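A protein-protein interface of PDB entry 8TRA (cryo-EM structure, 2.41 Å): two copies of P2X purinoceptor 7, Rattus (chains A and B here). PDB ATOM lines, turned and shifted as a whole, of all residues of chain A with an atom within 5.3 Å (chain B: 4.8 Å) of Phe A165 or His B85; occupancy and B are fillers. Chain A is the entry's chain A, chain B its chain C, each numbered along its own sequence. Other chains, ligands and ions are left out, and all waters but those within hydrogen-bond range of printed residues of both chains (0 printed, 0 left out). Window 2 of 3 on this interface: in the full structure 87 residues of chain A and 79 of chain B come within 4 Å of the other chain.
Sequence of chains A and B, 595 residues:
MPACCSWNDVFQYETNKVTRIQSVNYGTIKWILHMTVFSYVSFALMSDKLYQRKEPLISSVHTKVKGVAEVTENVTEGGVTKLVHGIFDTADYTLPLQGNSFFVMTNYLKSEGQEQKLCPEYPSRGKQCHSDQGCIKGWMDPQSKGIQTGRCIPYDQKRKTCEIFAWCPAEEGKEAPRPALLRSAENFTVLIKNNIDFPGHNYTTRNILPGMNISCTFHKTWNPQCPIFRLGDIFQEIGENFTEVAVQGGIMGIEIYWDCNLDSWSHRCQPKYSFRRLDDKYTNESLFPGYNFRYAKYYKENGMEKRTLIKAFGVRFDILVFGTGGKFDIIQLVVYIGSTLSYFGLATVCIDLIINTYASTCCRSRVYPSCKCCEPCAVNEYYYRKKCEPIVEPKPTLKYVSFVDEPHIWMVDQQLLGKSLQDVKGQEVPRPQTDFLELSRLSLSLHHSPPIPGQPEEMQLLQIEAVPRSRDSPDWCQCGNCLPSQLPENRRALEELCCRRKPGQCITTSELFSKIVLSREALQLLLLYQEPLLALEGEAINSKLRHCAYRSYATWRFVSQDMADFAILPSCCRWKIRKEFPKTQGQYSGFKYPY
The backbone NH of Ile B87 is in hydrogen-bond range of the side-chain amide oxygen of Gln A116, 2.7 Å away.
O of Ile A147 is in hydrogen-bond range of N of Phe A165 (2.8 Å). The backbone NH of Gly B86 lies within hydrogen-bond range of the backbone carbonyl oxygen of Val B71 (2.9 Å).
Among the printed residues, merely in contact across the chains: Gln A116 with Gly B86 (3.2 Å), Phe A165 with Ile B87 (3.5 Å), Trp A167 with Ile B87 (3.5 Å), Phe A165 with His B85 (3.6 Å), Ile A147 with Ile B87 (3.7 Å) and Ile A147 with Glu B70 (3.8 Å).
Of chain B, only His B85 and Ile B87 come within 4 Å of Phe A165. His B85 touches just one residue of chain A: Phe A165. Printed residues of chain A within 4 Å of Ile B87: Gln A116, Ile A147, Phe A165 and Trp A167. Of the printed residues of chain B, Trp A167 touches Ile B87. Printed residues of chain B within 4 Å of Ile A147: Glu B70 and Ile B87. Printed residues of chain B within 4 Å of Gln A116: Gly B86 and Ile B87. Lys A117 touches none of the printed residues of chain B. The nearest residue of chain A that does not touch His B85 is Gln A116 (4.2 Å). The nearest printed residue of chain A that does not touch Ile B87 is Ala A166 (4.1 Å).
Of the 14 printed residues of chain A, 4 touch a printed residue of chain B. Of the 8 printed residues of chain B, 4 touch a printed residue of chain A. Hydrophobic or aromatic side chains of chain B that line the printed part of chain A: His B85 and Ile B87. Among the printed residues, no Asp or Glu carboxylate lies within 4 Å of a Lys or Arg side-chain nitrogen of the other chain.
No position is printed for both chains.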
ATOM      1  N   GLN A 116       7.027  23.301  14.898  1.00  0.00           N
ATOM      2  CA  GLN A 116       7.155  21.906  14.478  1.00  0.00           C
ATOM      3  C   GLN A 116       7.012  21.025  15.711  1.00  0.00           C
ATOM      4  O   GLN A 116       7.954  20.869  16.493  1.00  0.00           O
ATOM      5  CB  GLN A 116       8.491  21.678  13.779  1.00  0.00           C
ATOM      6  CG  GLN A 116       8.684  22.529  12.536  1.00  0.00           C
ATOM      7  CD  GLN A 116      10.023  22.293  11.865  1.00  0.00           C
ATOM      8  OE1 GLN A 116      10.179  21.363  11.076  1.00  0.00           O
ATOM      9  NE2 GLN A 116      10.998  23.140  12.177  1.00  0.00           N
ATOM     10  N   LYS A 117       5.833  20.445  15.893  1.00  0.00           N
ATOM     11  CA  LYS A 117       5.537  19.645  17.081  1.00  0.00           C
ATOM     12  C   LYS A 117       4.283  18.822  16.797  1.00  0.00           C
ATOM     13  O   LYS A 117       3.785  18.791  15.666  1.00  0.00           O
ATOM     14  CB  LYS A 117       5.371  20.535  18.314  1.00  0.00           C
ATOM     15  CG  LYS A 117       4.087  21.345  18.324  1.00  0.00           C
ATOM     16  CD  LYS A 117       4.188  22.536  19.264  1.00  0.00           C
ATOM     17  CE  LYS A 117       2.842  23.219  19.444  1.00  0.00           C
ATOM     18  NZ  LYS A 117       2.940  24.433  20.300  1.00  0.00           N
ATOM     19  N   LEU A 118       3.775  18.152  17.828  1.00  0.00           N
ATOM     20  CA  LEU A 118       2.594  17.314  17.710  1.00  0.00           C
ATOM     21  C   LEU A 118       1.331  18.132  17.948  1.00  0.00           C
ATOM     22  O   LEU A 118       1.316  19.070  18.750  1.00  0.00           O
ATOM     23  CB  LEU A 118       2.651  16.158  18.709  1.00  0.00           C
ATOM     24  CG  LEU A 118       3.825  15.194  18.549  1.00  0.00           C
ATOM     25  CD1 LEU A 118       3.986  14.334  19.792  1.00  0.00           C
ATOM     26  CD2 LEU A 118       3.625  14.330  17.320  1.00  0.00           C
ATOM     27  N   CYS A 119       0.267  17.769  17.242  1.00  0.00           N
ATOM     28  CA  CYS A 119      -1.013  18.449  17.388  1.00  0.00           C
ATOM     29  C   CYS A 119      -2.090  17.612  16.704  1.00  0.00           C
ATOM     30  O   CYS A 119      -1.783  16.809  15.822  1.00  0.00           O
ATOM     31  CB  CYS A 119      -0.973  19.856  16.778  1.00  0.00           C
ATOM     32  SG  CYS A 119      -0.255  19.900  15.125  1.00  0.00           S
ATOM     33  N   LYS A 145      -0.847  17.244   5.947  1.00  0.00           N
ATOM     34  CA  LYS A 145       0.499  17.817   5.929  1.00  0.00           C
ATOM     35  C   LYS A 145       1.247  17.496   7.224  1.00  0.00           C
ATOM     36  O   LYS A 145       1.859  18.364   7.846  1.00  0.00           O
ATOM     37  CB  LYS A 145       0.442  19.327   5.682  1.00  0.00           C
ATOM     38  CG  LYS A 145      -0.389  19.702   4.468  1.00  0.00           C
ATOM     39  CD  LYS A 145       0.161  20.917   3.750  1.00  0.00           C
ATOM     40  CE  LYS A 145      -0.432  21.052   2.357  1.00  0.00           C
ATOM     41  NZ  LYS A 145      -1.901  20.811   2.343  1.00  0.00           N
ATOM     42  N   GLY A 146       1.178  16.247   7.656  1.00  0.00           N
ATOM     43  CA  GLY A 146       1.844  15.854   8.878  1.00  0.00           C
ATOM     44  C   GLY A 146       2.037  14.369   8.941  1.00  0.00           C
ATOM     45  O   GLY A 146       1.470  13.637   8.138  1.00  0.00           O
ATOM     46  N   ILE A 147       2.840  13.918   9.889  1.00  0.00           N
ATOM     47  CA  ILE A 147       3.103  12.495  10.044  1.00  0.00           C
ATOM     48  C   ILE A 147       2.349  11.982  11.249  1.00  0.00           C
ATOM     49  O   ILE A 147       2.561  12.454  12.357  1.00  0.00           O
ATOM     50  CB  ILE A 147       4.595  12.203  10.261  1.00  0.00           C
ATOM     51  CG1 ILE A 147       5.473  13.234   9.540  1.00  0.00           C
ATOM     52  CG2 ILE A 147       4.919  10.788   9.806  1.00  0.00           C
ATOM     53  CD1 ILE A 147       5.194  13.364   8.062  1.00  0.00           C
ATOM     54  N   GLN A 148       1.478  11.011  11.046  1.00  0.00           N
ATOM     55  CA  GLN A 148       0.659  10.513  12.145  1.00  0.00           C
ATOM     56  C   GLN A 148       1.444   9.740  13.191  1.00  0.00           C
ATOM     57  O   GLN A 148       2.420   9.081  12.865  1.00  0.00           O
ATOM     58  CB  GLN A 148      -0.452   9.628  11.601  1.00  0.00           C
ATOM     59  CG  GLN A 148      -1.446  10.378  10.737  1.00  0.00           C
ATOM     60  CD  GLN A 148      -2.670   9.553  10.411  1.00  0.00           C
ATOM     61  OE1 GLN A 148      -2.713   8.354  10.668  1.00  0.00           O
ATOM     62  NE2 GLN A 148      -3.671  10.197   9.830  1.00  0.00           N
ATOM     63  N   THR A 149       1.042   9.849  14.454  1.00  0.00           N
ATOM     64  CA  THR A 149       1.677   9.090  15.523  1.00  0.00           C
ATOM     65  C   THR A 149       0.866   7.870  15.940  1.00  0.00           C
ATOM     66  O   THR A 149       1.246   7.189  16.897  1.00  0.00           O
ATOM     67  CB  THR A 149       1.911   9.986  16.743  1.00  0.00           C
ATOM     68  OG1 THR A 149       0.651  10.387  17.297  1.00  0.00           O
ATOM     69  CG2 THR A 149       2.711  11.217  16.358  1.00  0.00           C
ATOM     70  N   GLU A 163      -3.414  12.490  16.081  1.00  0.00           N
ATOM     71  CA  GLU A 163      -2.242  13.321  16.319  1.00  0.00           C
ATOM     72  C   GLU A 163      -1.284  13.235  15.139  1.00  0.00           C
ATOM     73  O   GLU A 163      -1.121  12.176  14.527  1.00  0.00           O
ATOM     74  CB  GLU A 163      -1.537  12.880  17.601  1.00  0.00           C
ATOM     75  CG  GLU A 163      -0.162  13.495  17.800  1.00  0.00           C
ATOM     76  CD  GLU A 163       0.326  13.379  19.230  1.00  0.00           C
ATOM     77  OE1 GLU A 163      -0.034  14.247  20.054  1.00  0.00           O
ATOM     78  OE2 GLU A 163       1.066  12.420  19.532  1.00  0.00           O
ATOM     79  N   ILE A 164      -0.599  14.336  14.836  1.00  0.00           N
ATOM     80  CA  ILE A 164       0.379  14.343  13.756  1.00  0.00           C
ATOM     81  C   ILE A 164       1.532  15.263  14.073  1.00  0.00           C
ATOM     82  O   ILE A 164       1.345  16.276  14.737  1.00  0.00           O
ATOM     83  CB  ILE A 164      -0.234  14.819  12.425  1.00  0.00           C
ATOM     84  CG1 ILE A 164      -1.052  16.092  12.636  1.00  0.00           C
ATOM     85  CG2 ILE A 164      -1.107  13.736  11.822  1.00  0.00           C
ATOM     86  CD1 ILE A 164      -1.400  16.804  11.350  1.00  0.00           C
ATOM     87  N   PHE A 165       2.731  14.920  13.618  1.00  0.00           N
ATOM     88  CA  PHE A 165       3.860  15.823  13.784  1.00  0.00           C
ATOM     89  C   PHE A 165       3.795  16.766  12.609  1.00  0.00           C
ATOM     90  O   PHE A 165       3.795  16.324  11.463  1.00  0.00           O
ATOM     91  CB  PHE A 165       5.191  15.089  13.807  1.00  0.00           C
ATOM     92  CG  PHE A 165       6.377  16.006  13.847  1.00  0.00           C
ATOM     93  CD1 PHE A 165       6.617  16.791  14.958  1.00  0.00           C
ATOM     94  CD2 PHE A 165       7.251  16.087  12.775  1.00  0.00           C
ATOM     95  CE1 PHE A 165       7.705  17.641  15.002  1.00  0.00           C
ATOM     96  CE2 PHE A 165       8.341  16.933  12.813  1.00  0.00           C
ATOM     97  CZ  PHE A 165       8.568  17.711  13.930  1.00  0.00           C
ATOM     98  N   ALA A 166       3.742  18.063  12.873  1.00  0.00           N
ATOM     99  CA  ALA A 166       3.571  19.018  11.800  1.00  0.00           C
ATOM    100  C   ALA A 166       3.719  20.423  12.305  1.00  0.00           C
ATOM    101  O   ALA A 166       4.103  20.627  13.447  1.00  0.00           O
ATOM    102  CB  ALA A 166       2.185  18.835  11.210  1.00  0.00           C
ATOM    103  N   TRP A 167       3.454  21.405  11.460  1.00  0.00           N
ATOM    104  CA  TRP A 167       3.437  22.784  11.918  1.00  0.00           C
ATOM    105  C   TRP A 167       2.127  22.945  12.663  1.00  0.00           C
ATOM    106  O   TRP A 167       1.070  22.700  12.094  1.00  0.00           O
ATOM    107  CB  TRP A 167       3.561  23.751  10.757  1.00  0.00           C
ATOM    108  CG  TRP A 167       4.924  23.802  10.165  1.00  0.00           C
ATOM    109  CD1 TRP A 167       5.376  23.099   9.091  1.00  0.00           C
ATOM    110  CD2 TRP A 167       6.022  24.602  10.613  1.00  0.00           C
ATOM    111  NE1 TRP A 167       6.686  23.411   8.839  1.00  0.00           N
ATOM    112  CE2 TRP A 167       7.107  24.334   9.759  1.00  0.00           C
ATOM    113  CE3 TRP A 167       6.189  25.521  11.653  1.00  0.00           C
ATOM    114  CZ2 TRP A 167       8.346  24.950   9.913  1.00  0.00           C
ATOM    115  CZ3 TRP A 167       7.419  26.130  11.805  1.00  0.00           C
ATOM    116  CH2 TRP A 167       8.482  25.844  10.940  1.00  0.00           C
ATOM    117  N   GLU B  70      10.215  14.154   6.143  1.00  0.00           N
ATOM    118  CA  GLU B  70      10.765  14.103   7.489  1.00  0.00           C
ATOM    119  C   GLU B  70      12.279  14.232   7.422  1.00  0.00           C
ATOM    120  O   GLU B  70      12.919  13.646   6.542  1.00  0.00           O
ATOM    121  CB  GLU B  70      10.390  12.785   8.174  1.00  0.00           C
ATOM    122  CG  GLU B  70       9.277  12.885   9.202  1.00  0.00           C
ATOM    123  CD  GLU B  70       9.444  11.890  10.333  1.00  0.00           C
ATOM    124  OE1 GLU B  70       9.782  12.310  11.457  1.00  0.00           O
ATOM    125  OE2 GLU B  70       9.237  10.680  10.094  1.00  0.00           O
ATOM    126  N   VAL B  71      12.857  14.997   8.347  1.00  0.00           N
ATOM    127  CA  VAL B  71      14.305  15.131   8.451  1.00  0.00           C
ATOM    128  C   VAL B  71      14.698  15.027   9.918  1.00  0.00           C
ATOM    129  O   VAL B  71      13.982  15.515  10.797  1.00  0.00           O
ATOM    130  CB  VAL B  71      14.803  16.461   7.844  1.00  0.00           C
ATOM    131  CG1 VAL B  71      16.305  16.624   8.053  1.00  0.00           C
ATOM    132  CG2 VAL B  71      14.469  16.524   6.363  1.00  0.00           C
ATOM    133  N   THR B  72      15.834  14.382  10.179  1.00  0.00           N
ATOM    134  CA  THR B  72      16.410  14.290  11.523  1.00  0.00           C
ATOM    135  C   THR B  72      17.889  14.627  11.379  1.00  0.00           C
ATOM    136  O   THR B  72      18.718  13.740  11.158  1.00  0.00           O
ATOM    137  CB  THR B  72      16.190  12.908  12.132  1.00  0.00           C
ATOM    138  OG1 THR B  72      14.839  12.487  11.899  1.00  0.00           O
ATOM    139  CG2 THR B  72      16.451  12.939  13.629  1.00  0.00           C
ATOM    140  N   LEU B  83      20.395  17.199  17.913  1.00  0.00           N
ATOM    141  CA  LEU B  83      19.589  16.510  16.912  1.00  0.00           C
ATOM    142  C   LEU B  83      18.264  17.239  16.737  1.00  0.00           C
ATOM    143  O   LEU B  83      17.454  17.303  17.668  1.00  0.00           O
ATOM    144  CB  LEU B  83      19.359  15.060  17.327  1.00  0.00           C
ATOM    145  CG  LEU B  83      18.795  14.129  16.251  1.00  0.00           C
ATOM    146  CD1 LEU B  83      19.770  13.991  15.091  1.00  0.00           C
ATOM    147  CD2 LEU B  83      18.464  12.766  16.840  1.00  0.00           C
ATOM    148  N   VAL B  84      18.039  17.786  15.544  1.00  0.00           N
ATOM    149  CA  VAL B  84      16.859  18.589  15.246  1.00  0.00           C
ATOM    150  C   VAL B  84      15.930  17.777  14.356  1.00  0.00           C
ATOM    151  O   VAL B  84      16.351  17.253  13.316  1.00  0.00           O
ATOM    152  CB  VAL B  84      17.235  19.920  14.573  1.00  0.00           C
ATOM    153  CG1 VAL B  84      15.989  20.758  14.319  1.00  0.00           C
ATOM    154  CG2 VAL B  84      18.232  20.684  15.429  1.00  0.00           C
ATOM    155  N   HIS B  85      14.669  17.675  14.770  1.00  0.00           N
ATOM    156  CA  HIS B  85      13.628  17.009  14.003  1.00  0.00           C
ATOM    157  C   HIS B  85      12.855  18.054  13.210  1.00  0.00           C
ATOM    158  O   HIS B  85      12.402  19.056  13.775  1.00  0.00           O
ATOM    159  CB  HIS B  85      12.688  16.238  14.932  1.00  0.00           C
ATOM    160  CG  HIS B  85      11.810  15.253  14.226  1.00  0.00           C
ATOM    161  ND1 HIS B  85      10.616  14.812  14.754  1.00  0.00           N
ATOM    162  CD2 HIS B  85      11.954  14.620  13.039  1.00  0.00           C
ATOM    163  CE1 HIS B  85      10.061  13.950  13.920  1.00  0.00           C
ATOM    164  NE2 HIS B  85      10.853  13.817  12.872  1.00  0.00           N
ATOM    165  N   GLY B  86      12.708  17.821  11.917  1.00  0.00           N
ATOM    166  CA  GLY B  86      12.115  18.808  11.029  1.00  0.00           C
ATOM    167  C   GLY B  86      11.070  18.206  10.118  1.00  0.00           C
ATOM    168  O   GLY B  86      11.230  17.093   9.611  1.00  0.00           O
ATOM    169  N   ILE B  87      10.001  18.966   9.902  1.00  0.00           N
ATOM    170  CA  ILE B  87       8.889  18.582   9.042  1.00  0.00           C
ATOM    171  C   ILE B  87       8.858  19.542   7.862  1.00  0.00           C
ATOM    172  O   ILE B  87       8.897  20.765   8.050  1.00  0.00           O
ATOM    173  CB  ILE B  87       7.554  18.600   9.809  1.00  0.00           C
ATOM    174  CG1 ILE B  87       6.390  18.244   8.884  1.00  0.00           C
ATOM    175  CG2 ILE B  87       7.312  19.962  10.453  1.00  0.00           C
ATOM    176  CD1 ILE B  87       6.473  16.854   8.329  1.00  0.00           C
